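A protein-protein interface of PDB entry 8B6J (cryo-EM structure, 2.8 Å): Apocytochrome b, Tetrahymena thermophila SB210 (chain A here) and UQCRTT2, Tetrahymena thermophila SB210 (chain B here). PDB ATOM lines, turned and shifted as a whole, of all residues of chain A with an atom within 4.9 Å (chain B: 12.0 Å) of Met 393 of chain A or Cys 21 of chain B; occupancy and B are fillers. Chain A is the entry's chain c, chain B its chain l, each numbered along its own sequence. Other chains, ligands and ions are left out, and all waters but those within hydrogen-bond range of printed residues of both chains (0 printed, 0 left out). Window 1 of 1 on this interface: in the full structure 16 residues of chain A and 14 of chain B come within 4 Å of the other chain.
The side-chain sulfur (SG) of Cys 21 of chain B lies close to the side-chain sulfur (SD) of Met 393 of chain A (3.7 Å).
The side-chain sulfur (SG) of Cys 21 of chain B sits at hydrogen-bond distance from the backbone carbonyl oxygen (O) of Pro 17 of chain B.
Among the printed residues, pairs that only touch across the chains: Leu 389 of chain A with Cys 21 of chain B (3.4 Å), Phe 397 of chain A with Tyr 14 of chain B (3.4 Å), Phe 397 of chain A with Pro 17 of chain B (3.5 Å) and Met 393 of chain A with Pro 17 of chain B (3.8 Å).
Of the printed residues of chain B, Leu 389 of chain A touches Cys 21. Ser 391 of chain A touches none of the printed residues of chain B. Phe 392 of chain A touches none of the printed residues of chain B. Met 393 of chain A touches just these residues of chain B: Pro 17 (3.8 Å) and Cys 21 (3.5 Å). Ile 395 of chain A touches none of the printed residues of chain B. Phe 397 of chain A touches just these residues of chain B: Tyr 14 (3.4 Å) and Pro 17 (3.5 Å). Printed residues of chain A within 4 Å of Tyr 14 of chain B: Phe 397 (3.4 Å). Tyr 16 of chain B touches none of the printed residues of chain A. Printed residues of chain A within 4 Å of Pro 17 of chain B: Met 393 (3.8 Å) and Phe 397 (3.5 Å). Cys 21 of chain B touches two residues of chain A. The nearest residue of chain B that does not touch Met 393 of chain A is Val 20 of chain B (4.1 Å). The nearest printed residue of chain A that does not touch Cys 21 of chain B is Trp 390 of chain A (6.7 Å). The nearest printed residue of chain A that does not touch Tyr 14 of chain B is Met 393 of chain A (8.4 Å).
Of the 10 printed residues of chain A, 3 touch a printed residue of chain B. Along chain A the printed residues that touch a printed residue of chain B span positions 389 to 397. Among the printed residues, 5 pairs touch across the chains. Among the printed residues, no Asp or Glu carboxylate lies within 4 Å of a Lys or Arg side-chain nitrogen of the other chain.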
ATOM      1  N   TRP A 288     -22.545 -23.308   5.175  1.00  0.00           N
ATOM      2  CA  TRP A 288     -21.550 -22.262   5.384  1.00  0.00           C
ATOM      3  C   TRP A 288     -20.874 -21.881   4.076  1.00  0.00           C
ATOM      4  O   TRP A 288     -20.666 -20.695   3.796  1.00  0.00           O
ATOM      5  CB  TRP A 288     -20.515 -22.725   6.409  1.00  0.00           C
ATOM      6  CG  TRP A 288     -19.319 -21.830   6.517  1.00  0.00           C
ATOM      7  CD1 TRP A 288     -18.021 -22.173   6.287  1.00  0.00           C
ATOM      8  CD2 TRP A 288     -19.311 -20.446   6.882  1.00  0.00           C
ATOM      9  NE1 TRP A 288     -17.202 -21.090   6.488  1.00  0.00           N
ATOM     10  CE2 TRP A 288     -17.970 -20.016   6.853  1.00  0.00           C
ATOM     11  CE3 TRP A 288     -20.305 -19.528   7.229  1.00  0.00           C
ATOM     12  CZ2 TRP A 288     -17.600 -18.710   7.158  1.00  0.00           C
ATOM     13  CZ3 TRP A 288     -19.935 -18.233   7.532  1.00  0.00           C
ATOM     14  CH2 TRP A 288     -18.595 -17.836   7.494  1.00  0.00           C
ATOM     15  N   LEU A 389     -26.952 -16.296   8.969  1.00  0.00           N
ATOM     16  CA  LEU A 389     -25.765 -15.483   9.207  1.00  0.00           C
ATOM     17  C   LEU A 389     -25.597 -15.186  10.689  1.00  0.00           C
ATOM     18  O   LEU A 389     -24.487 -15.274  11.229  1.00  0.00           O
ATOM     19  CB  LEU A 389     -25.856 -14.184   8.406  1.00  0.00           C
ATOM     20  CG  LEU A 389     -24.577 -13.741   7.697  1.00  0.00           C
ATOM     21  CD1 LEU A 389     -24.821 -12.461   6.920  1.00  0.00           C
ATOM     22  CD2 LEU A 389     -23.443 -13.559   8.687  1.00  0.00           C
ATOM     23  N   TRP A 390     -26.693 -14.840  11.369  1.00  0.00           N
ATOM     24  CA  TRP A 390     -26.621 -14.573  12.800  1.00  0.00           C
ATOM     25  C   TRP A 390     -26.138 -15.800  13.560  1.00  0.00           C
ATOM     26  O   TRP A 390     -25.281 -15.694  14.443  1.00  0.00           O
ATOM     27  CB  TRP A 390     -27.990 -14.127  13.312  1.00  0.00           C
ATOM     28  CG  TRP A 390     -28.085 -13.978  14.804  1.00  0.00           C
ATOM     29  CD1 TRP A 390     -27.099 -13.576  15.656  1.00  0.00           C
ATOM     30  CD2 TRP A 390     -29.237 -14.236  15.618  1.00  0.00           C
ATOM     31  NE1 TRP A 390     -27.565 -13.565  16.949  1.00  0.00           N
ATOM     32  CE2 TRP A 390     -28.875 -13.966  16.952  1.00  0.00           C
ATOM     33  CE3 TRP A 390     -30.542 -14.666  15.346  1.00  0.00           C
ATOM     34  CZ2 TRP A 390     -29.769 -14.112  18.012  1.00  0.00           C
ATOM     35  CZ3 TRP A 390     -31.426 -14.811  16.400  1.00  0.00           C
ATOM     36  CH2 TRP A 390     -31.037 -14.536  17.716  1.00  0.00           C
ATOM     37  N   SER A 391     -26.674 -16.976  13.228  1.00  0.00           N
ATOM     38  CA  SER A 391     -26.281 -18.193  13.928  1.00  0.00           C
ATOM     39  C   SER A 391     -24.817 -18.530  13.677  1.00  0.00           C
ATOM     40  O   SER A 391     -24.097 -18.907  14.607  1.00  0.00           O
ATOM     41  CB  SER A 391     -27.182 -19.350  13.505  1.00  0.00           C
ATOM     42  OG  SER A 391     -27.188 -19.502  12.098  1.00  0.00           O
ATOM     43  N   PHE A 392     -24.352 -18.400  12.432  1.00  0.00           N
ATOM     44  CA  PHE A 392     -22.948 -18.682  12.145  1.00  0.00           C
ATOM     45  C   PHE A 392     -22.032 -17.729  12.901  1.00  0.00           C
ATOM     46  O   PHE A 392     -21.028 -18.146  13.493  1.00  0.00           O
ATOM     47  CB  PHE A 392     -22.687 -18.586  10.642  1.00  0.00           C
ATOM     48  CG  PHE A 392     -22.947 -19.860   9.898  1.00  0.00           C
ATOM     49  CD1 PHE A 392     -22.198 -20.992  10.156  1.00  0.00           C
ATOM     50  CD2 PHE A 392     -23.929 -19.922   8.926  1.00  0.00           C
ATOM     51  CE1 PHE A 392     -22.430 -22.162   9.474  1.00  0.00           C
ATOM     52  CE2 PHE A 392     -24.165 -21.092   8.237  1.00  0.00           C
ATOM     53  CZ  PHE A 392     -23.414 -22.212   8.511  1.00  0.00           C
ATOM     54  N   MET A 393     -22.360 -16.437  12.891  1.00  0.00           N
ATOM     55  CA  MET A 393     -21.504 -15.469  13.564  1.00  0.00           C
ATOM     56  C   MET A 393     -21.524 -15.672  15.072  1.00  0.00           C
ATOM     57  O   MET A 393     -20.496 -15.505  15.737  1.00  0.00           O
ATOM     58  CB  MET A 393     -21.930 -14.052  13.194  1.00  0.00           C
ATOM     59  CG  MET A 393     -21.731 -13.740  11.721  1.00  0.00           C
ATOM     60  SD  MET A 393     -20.008 -13.896  11.209  1.00  0.00           S
ATOM     61  CE  MET A 393     -20.192 -14.267   9.468  1.00  0.00           C
ATOM     62  N   TYR A 394     -22.675 -16.044  15.635  1.00  0.00           N
ATOM     63  CA  TYR A 394     -22.716 -16.325  17.063  1.00  0.00           C
ATOM     64  C   TYR A 394     -21.950 -17.595  17.403  1.00  0.00           C
ATOM     65  O   TYR A 394     -21.362 -17.686  18.483  1.00  0.00           O
ATOM     66  CB  TYR A 394     -24.157 -16.435  17.554  1.00  0.00           C
ATOM     67  CG  TYR A 394     -24.245 -16.529  19.057  1.00  0.00           C
ATOM     68  CD1 TYR A 394     -24.194 -15.390  19.846  1.00  0.00           C
ATOM     69  CD2 TYR A 394     -24.357 -17.757  19.690  1.00  0.00           C
ATOM     70  CE1 TYR A 394     -24.263 -15.470  21.221  1.00  0.00           C
ATOM     71  CE2 TYR A 394     -24.427 -17.846  21.064  1.00  0.00           C
ATOM     72  CZ  TYR A 394     -24.379 -16.700  21.823  1.00  0.00           C
ATOM     73  OH  TYR A 394     -24.450 -16.788  23.193  1.00  0.00           O
ATOM     74  N   ILE A 395     -21.950 -18.584  16.508  1.00  0.00           N
ATOM     75  CA  ILE A 395     -21.127 -19.770  16.724  1.00  0.00           C
ATOM     76  C   ILE A 395     -19.655 -19.388  16.750  1.00  0.00           C
ATOM     77  O   ILE A 395     -18.893 -19.846  17.609  1.00  0.00           O
ATOM     78  CB  ILE A 395     -21.416 -20.825  15.642  1.00  0.00           C
ATOM     79  CG1 ILE A 395     -22.794 -21.446  15.866  1.00  0.00           C
ATOM     80  CG2 ILE A 395     -20.335 -21.896  15.642  1.00  0.00           C
ATOM     81  CD1 ILE A 395     -23.304 -22.235  14.686  1.00  0.00           C
ATOM     82  N   PHE A 396     -19.231 -18.547  15.805  1.00  0.00           N
ATOM     83  CA  PHE A 396     -17.835 -18.118  15.780  1.00  0.00           C
ATOM     84  C   PHE A 396     -17.474 -17.327  17.031  1.00  0.00           C
ATOM     85  O   PHE A 396     -16.402 -17.526  17.611  1.00  0.00           O
ATOM     86  CB  PHE A 396     -17.561 -17.286  14.527  1.00  0.00           C
ATOM     87  CG  PHE A 396     -17.677 -18.057  13.244  1.00  0.00           C
ATOM     88  CD1 PHE A 396     -17.251 -19.373  13.163  1.00  0.00           C
ATOM     89  CD2 PHE A 396     -18.212 -17.465  12.116  1.00  0.00           C
ATOM     90  CE1 PHE A 396     -17.360 -20.077  11.982  1.00  0.00           C
ATOM     91  CE2 PHE A 396     -18.321 -18.166  10.934  1.00  0.00           C
ATOM     92  CZ  PHE A 396     -17.896 -19.471  10.868  1.00  0.00           C
ATOM     93  N   PHE A 397     -18.354 -16.420  17.460  1.00  0.00           N
ATOM     94  CA  PHE A 397     -18.050 -15.595  18.626  1.00  0.00           C
ATOM     95  C   PHE A 397     -18.041 -16.416  19.909  1.00  0.00           C
ATOM     96  O   PHE A 397     -17.148 -16.255  20.748  1.00  0.00           O
ATOM     97  CB  PHE A 397     -19.055 -14.451  18.737  1.00  0.00           C
ATOM     98  CG  PHE A 397     -18.614 -13.190  18.054  1.00  0.00           C
ATOM     99  CD1 PHE A 397     -18.897 -12.973  16.719  1.00  0.00           C
ATOM    100  CD2 PHE A 397     -17.914 -12.221  18.752  1.00  0.00           C
ATOM    101  CE1 PHE A 397     -18.490 -11.814  16.092  1.00  0.00           C
ATOM    102  CE2 PHE A 397     -17.505 -11.060  18.130  1.00  0.00           C
ATOM    103  CZ  PHE A 397     -17.794 -10.856  16.798  1.00  0.00           C
ATOM    104  N   VAL B  12      -8.683  -7.259  15.998  1.00  0.00           N
ATOM    105  CA  VAL B  12      -8.904  -8.052  14.793  1.00  0.00           C
ATOM    106  C   VAL B  12      -9.851  -9.207  15.086  1.00  0.00           C
ATOM    107  O   VAL B  12     -10.766  -9.492  14.305  1.00  0.00           O
ATOM    108  CB  VAL B  12      -7.561  -8.550  14.230  1.00  0.00           C
ATOM    109  CG1 VAL B  12      -7.793  -9.573  13.130  1.00  0.00           C
ATOM    110  CG2 VAL B  12      -6.746  -7.382  13.704  1.00  0.00           C
ATOM    111  N   ILE B  13      -9.652  -9.886  16.217  1.00  0.00           N
ATOM    112  CA  ILE B  13     -10.528 -10.996  16.578  1.00  0.00           C
ATOM    113  C   ILE B  13     -11.968 -10.516  16.694  1.00  0.00           C
ATOM    114  O   ILE B  13     -12.896 -11.167  16.201  1.00  0.00           O
ATOM    115  CB  ILE B  13     -10.047 -11.651  17.886  1.00  0.00           C
ATOM    116  CG1 ILE B  13      -8.720 -12.377  17.659  1.00  0.00           C
ATOM    117  CG2 ILE B  13     -11.099 -12.612  18.417  1.00  0.00           C
ATOM    118  CD1 ILE B  13      -7.998 -12.748  18.938  1.00  0.00           C
ATOM    119  N   TYR B  14     -12.179  -9.374  17.350  1.00  0.00           N
ATOM    120  CA  TYR B  14     -13.539  -8.863  17.502  1.00  0.00           C
ATOM    121  C   TYR B  14     -14.139  -8.445  16.164  1.00  0.00           C
ATOM    122  O   TYR B  14     -15.319  -8.703  15.903  1.00  0.00           O
ATOM    123  CB  TYR B  14     -13.559  -7.681  18.474  1.00  0.00           C
ATOM    124  CG  TYR B  14     -13.599  -8.038  19.949  1.00  0.00           C
ATOM    125  CD1 TYR B  14     -14.074  -9.268  20.390  1.00  0.00           C
ATOM    126  CD2 TYR B  14     -13.170  -7.128  20.904  1.00  0.00           C
ATOM    127  CE1 TYR B  14     -14.111  -9.580  21.732  1.00  0.00           C
ATOM    128  CE2 TYR B  14     -13.204  -7.433  22.249  1.00  0.00           C
ATOM    129  CZ  TYR B  14     -13.675  -8.661  22.657  1.00  0.00           C
ATOM    130  OH  TYR B  14     -13.710  -8.970  23.996  1.00  0.00           O
ATOM    131  N   SER B  15     -13.351  -7.800  15.301  1.00  0.00           N
ATOM    132  CA  SER B  15     -13.906  -7.099  14.152  1.00  0.00           C
ATOM    133  C   SER B  15     -13.924  -7.910  12.863  1.00  0.00           C
ATOM    134  O   SER B  15     -14.651  -7.535  11.937  1.00  0.00           O
ATOM    135  CB  SER B  15     -13.121  -5.805  13.901  1.00  0.00           C
ATOM    136  OG  SER B  15     -11.763  -6.080  13.616  1.00  0.00           O
ATOM    137  N   TYR B  16     -13.155  -8.993  12.760  1.00  0.00           N
ATOM    138  CA  TYR B  16     -13.113  -9.722  11.497  1.00  0.00           C
ATOM    139  C   TYR B  16     -14.460 -10.315  11.106  1.00  0.00           C
ATOM    140  O   TYR B  16     -14.822 -10.214   9.920  1.00  0.00           O
ATOM    141  CB  TYR B  16     -12.038 -10.815  11.551  1.00  0.00           C
ATOM    142  CG  TYR B  16     -11.829 -11.483  10.214  1.00  0.00           C
ATOM    143  CD1 TYR B  16     -11.199 -10.812   9.176  1.00  0.00           C
ATOM    144  CD2 TYR B  16     -12.271 -12.777   9.984  1.00  0.00           C
ATOM    145  CE1 TYR B  16     -11.011 -11.412   7.951  1.00  0.00           C
ATOM    146  CE2 TYR B  16     -12.087 -13.385   8.760  1.00  0.00           C
ATOM    147  CZ  TYR B  16     -11.457 -12.697   7.747  1.00  0.00           C
ATOM    148  OH  TYR B  16     -11.269 -13.299   6.525  1.00  0.00           O
ATOM    149  N   PRO B  17     -15.225 -10.948  12.000  1.00  0.00           N
ATOM    150  CA  PRO B  17     -16.551 -11.434  11.585  1.00  0.00           C
ATOM    151  C   PRO B  17     -17.442 -10.336  11.031  1.00  0.00           C
ATOM    152  O   PRO B  17     -18.206 -10.576  10.089  1.00  0.00           O
ATOM    153  CB  PRO B  17     -17.119 -12.037  12.878  1.00  0.00           C
ATOM    154  CG  PRO B  17     -15.923 -12.394  13.683  1.00  0.00           C
ATOM    155  CD  PRO B  17     -14.902 -11.341  13.382  1.00  0.00           C
ATOM    156  N   LEU B  18     -17.364  -9.128  11.590  1.00  0.00           N
ATOM    157  CA  LEU B  18     -18.134  -8.017  11.042  1.00  0.00           C
ATOM    158  C   LEU B  18     -17.685  -7.689   9.624  1.00  0.00           C
ATOM    159  O   LEU B  18     -18.511  -7.381   8.758  1.00  0.00           O
ATOM    160  CB  LEU B  18     -18.002  -6.794  11.949  1.00  0.00           C
ATOM    161  CG  LEU B  18     -18.336  -7.025  13.424  1.00  0.00           C
ATOM    162  CD1 LEU B  18     -18.215  -5.727  14.206  1.00  0.00           C
ATOM    163  CD2 LEU B  18     -19.725  -7.618  13.582  1.00  0.00           C
ATOM    164  N   TYR B  19     -16.376  -7.744   9.370  1.00  0.00           N
ATOM    165  CA  TYR B  19     -15.883  -7.525   8.014  1.00  0.00           C
ATOM    166  C   TYR B  19     -16.389  -8.605   7.067  1.00  0.00           C
ATOM    167  O   TYR B  19     -16.737  -8.320   5.914  1.00  0.00           O
ATOM    168  CB  TYR B  19     -14.355  -7.483   8.016  1.00  0.00           C
ATOM    169  CG  TYR B  19     -13.750  -7.259   6.651  1.00  0.00           C
ATOM    170  CD1 TYR B  19     -13.863  -6.032   6.014  1.00  0.00           C
ATOM    171  CD2 TYR B  19     -13.062  -8.272   6.000  1.00  0.00           C
ATOM    172  CE1 TYR B  19     -13.313  -5.821   4.767  1.00  0.00           C
ATOM    173  CE2 TYR B  19     -12.507  -8.071   4.753  1.00  0.00           C
ATOM    174  CZ  TYR B  19     -12.635  -6.844   4.140  1.00  0.00           C
ATOM    175  OH  TYR B  19     -12.083  -6.638   2.898  1.00  0.00           O
ATOM    176  N   VAL B  20     -16.437  -9.853   7.534  1.00  0.00           N
ATOM    177  CA  VAL B  20     -16.973 -10.931   6.707  1.00  0.00           C
ATOM    178  C   VAL B  20     -18.442 -10.678   6.393  1.00  0.00           C
ATOM    179  O   VAL B  20     -18.899 -10.899   5.266  1.00  0.00           O
ATOM    180  CB  VAL B  20     -16.770 -12.291   7.400  1.00  0.00           C
ATOM    181  CG1 VAL B  20     -17.422 -13.400   6.592  1.00  0.00           C
ATOM    182  CG2 VAL B  20     -15.291 -12.571   7.591  1.00  0.00           C
ATOM    183  N   CYS B  21     -19.209 -10.227   7.389  1.00  0.00           N
ATOM    184  CA  CYS B  21     -20.615  -9.909   7.154  1.00  0.00           C
ATOM    185  C   CYS B  21     -20.760  -8.779   6.142  1.00  0.00           C
ATOM    186  O   CYS B  21     -21.647  -8.814   5.282  1.00  0.00           O
ATOM    187  CB  CYS B  21     -21.298  -9.535   8.468  1.00  0.00           C
ATOM    188  SG  CYS B  21     -21.530 -10.911   9.605  1.00  0.00           S
ATOM    189  N   TYR B  22     -19.908  -7.759   6.242  1.00  0.00           N
ATOM    190  CA  TYR B  22     -19.936  -6.673   5.269  1.00  0.00           C
ATOM    191  C   TYR B  22     -19.638  -7.187   3.866  1.00  0.00           C
ATOM    192  O   TYR B  22     -20.301  -6.798   2.896  1.00  0.00           O
ATOM    193  CB  TYR B  22     -18.933  -5.592   5.670  1.00  0.00           C
ATOM    194  CG  TYR B  22     -18.777  -4.485   4.655  1.00  0.00           C
ATOM    195  CD1 TYR B  22     -19.617  -3.382   4.669  1.00  0.00           C
ATOM    196  CD2 TYR B  22     -17.785  -4.540   3.686  1.00  0.00           C
ATOM    197  CE1 TYR B  22     -19.476  -2.367   3.745  1.00  0.00           C
ATOM    198  CE2 TYR B  22     -17.638  -3.530   2.757  1.00  0.00           C
ATOM    199  CZ  TYR B  22     -18.486  -2.446   2.791  1.00  0.00           C
ATOM    200  OH  TYR B  22     -18.342  -1.437   1.868  1.00  0.00           O
ATOM    201  N   LEU B  23     -18.644  -8.068   3.740  1.00  0.00           N
ATOM    202  CA  LEU B  23     -18.330  -8.641   2.435  1.00  0.00           C
ATOM    203  C   LEU B  23     -19.503  -9.449   1.897  1.00  0.00           C
ATOM    204  O   LEU B  23     -19.809  -9.390   0.701  1.00  0.00           O
ATOM    205  CB  LEU B  23     -17.083  -9.518   2.527  1.00  0.00           C
ATOM    206  CG  LEU B  23     -15.741  -8.833   2.801  1.00  0.00           C
ATOM    207  CD1 LEU B  23     -14.617  -9.851   2.725  1.00  0.00           C
ATOM    208  CD2 LEU B  23     -15.493  -7.689   1.834  1.00  0.00           C
ATOM    209  N   ILE B  24     -20.167 -10.216   2.763  1.00  0.00           N
ATOM    210  CA  ILE B  24     -21.315 -11.009   2.330  1.00  0.00           C
ATOM    211  C   ILE B  24     -22.443 -10.102   1.855  1.00  0.00           C
ATOM    212  O   ILE B  24     -23.100 -10.379   0.845  1.00  0.00           O
ATOM    213  CB  ILE B  24     -21.778 -11.939   3.468  1.00  0.00           C
ATOM    214  CG1 ILE B  24     -20.719 -13.011   3.735  1.00  0.00           C
ATOM    215  CG2 ILE B  24     -23.111 -12.579   3.118  1.00  0.00           C
ATOM    216  CD1 ILE B  24     -20.937 -13.786   5.014  1.00  0.00           C
ATOM    217  N   LYS B  25     -22.699  -9.016   2.585  1.00  0.00           N
ATOM    218  CA  LYS B  25     -23.744  -8.084   2.173  1.00  0.00           C
ATOM    219  C   LYS B  25     -23.412  -7.451   0.829  1.00  0.00           C
ATOM    220  O   LYS B  25     -24.288  -7.307  -0.035  1.00  0.00           O
ATOM    221  CB  LYS B  25     -23.938  -7.010   3.244  1.00  0.00           C
ATOM    222  CG  LYS B  25     -25.034  -6.000   2.933  1.00  0.00           C
ATOM    223  CD  LYS B  25     -26.397  -6.662   2.803  1.00  0.00           C
ATOM    224  CE  LYS B  25     -27.490  -5.640   2.533  1.00  0.00           C
ATOM    225  NZ  LYS B  25     -28.827  -6.277   2.383  1.00  0.00           N
ATOM    226  N   GLN B  26     -22.152  -7.060   0.633  1.00  0.00           N
ATOM    227  CA  GLN B  26     -21.754  -6.504  -0.656  1.00  0.00           C
ATOM    228  C   GLN B  26     -21.909  -7.533  -1.767  1.00  0.00           C
ATOM    229  O   GLN B  26     -22.324  -7.197  -2.882  1.00  0.00           O
ATOM    230  CB  GLN B  26     -20.314  -5.996  -0.587  1.00  0.00           C
ATOM    231  CG  GLN B  26     -20.127  -4.810   0.339  1.00  0.00           C
ATOM    232  CD  GLN B  26     -20.977  -3.622  -0.062  1.00  0.00           C
ATOM    233  OE1 GLN B  26     -21.350  -3.476  -1.225  1.00  0.00           O
ATOM    234  NE2 GLN B  26     -21.297  -2.770   0.904  1.00  0.00           N
ATOM    235  N   ALA B  27     -21.577  -8.793  -1.483  1.00  0.00           N
ATOM    236  CA  ALA B  27     -21.748  -9.845  -2.478  1.00  0.00           C
ATOM    237  C   ALA B  27     -23.215 -10.015  -2.847  1.00  0.00           C
ATOM    238  O   ALA B  27     -23.549 -10.201  -4.021  1.00  0.00           O
ATOM    239  CB  ALA B  27     -21.170 -11.160  -1.958  1.00  0.00           C
ATOM    240  N   GLN B  28     -24.106  -9.962  -1.856  1.00  0.00           N
ATOM    241  CA  GLN B  28     -25.535 -10.057  -2.144  1.00  0.00           C
ATOM    242  C   GLN B  28     -25.998  -8.886  -3.004  1.00  0.00           C
ATOM    243  O   GLN B  28     -26.734  -9.067  -3.984  1.00  0.00           O
ATOM    244  CB  GLN B  28     -26.330 -10.110  -0.840  1.00  0.00           C
ATOM    245  CG  GLN B  28     -26.115 -11.375  -0.034  1.00  0.00           C
ATOM    246  CD  GLN B  28     -26.807 -11.327   1.310  1.00  0.00           C
ATOM    247  OE1 GLN B  28     -27.400 -10.314   1.677  1.00  0.00           O
ATOM    248  NE2 GLN B  28     -26.734 -12.422   2.052  1.00  0.00           N
ATOM    249  N   ILE B  29     -25.567  -7.672  -2.655  1.00  0.00           N
ATOM    250  CA  ILE B  29     -25.965  -6.500  -3.430  1.00  0.00           C
ATOM    251  C   ILE B  29     -25.472  -6.624  -4.865  1.00  0.00           C
ATOM    252  O   ILE B  29     -26.186  -6.279  -5.814  1.00  0.00           O
ATOM    253  CB  ILE B  29     -25.449  -5.212  -2.760  1.00  0.00           C
ATOM    254  CG1 ILE B  29     -26.156  -5.000  -1.419  1.00  0.00           C
ATOM    255  CG2 ILE B  29     -25.662  -4.017  -3.682  1.00  0.00           C
ATOM    256  CD1 ILE B  29     -25.607  -3.850  -0.605  1.00  0.00           C
ATOM    257  N   ASN B  30     -24.243  -7.110  -5.047  1.00  0.00           N
ATOM    258  CA  ASN B  30     -23.732  -7.336  -6.394  1.00  0.00           C
ATOM    259  C   ASN B  30     -24.561  -8.386  -7.125  1.00  0.00           C
ATOM    260  O   ASN B  30     -24.883  -8.221  -8.307  1.00  0.00           O
ATOM    261  CB  ASN B  30     -22.267  -7.761  -6.330  1.00  0.00           C
ATOM    262  CG  ASN B  30     -21.384  -6.716  -5.677  1.00  0.00           C
ATOM    263  OD1 ASN B  30     -21.876  -5.780  -5.046  1.00  0.00           O
ATOM    264  ND2 ASN B  30     -20.074  -6.874  -5.824  1.00  0.00           N
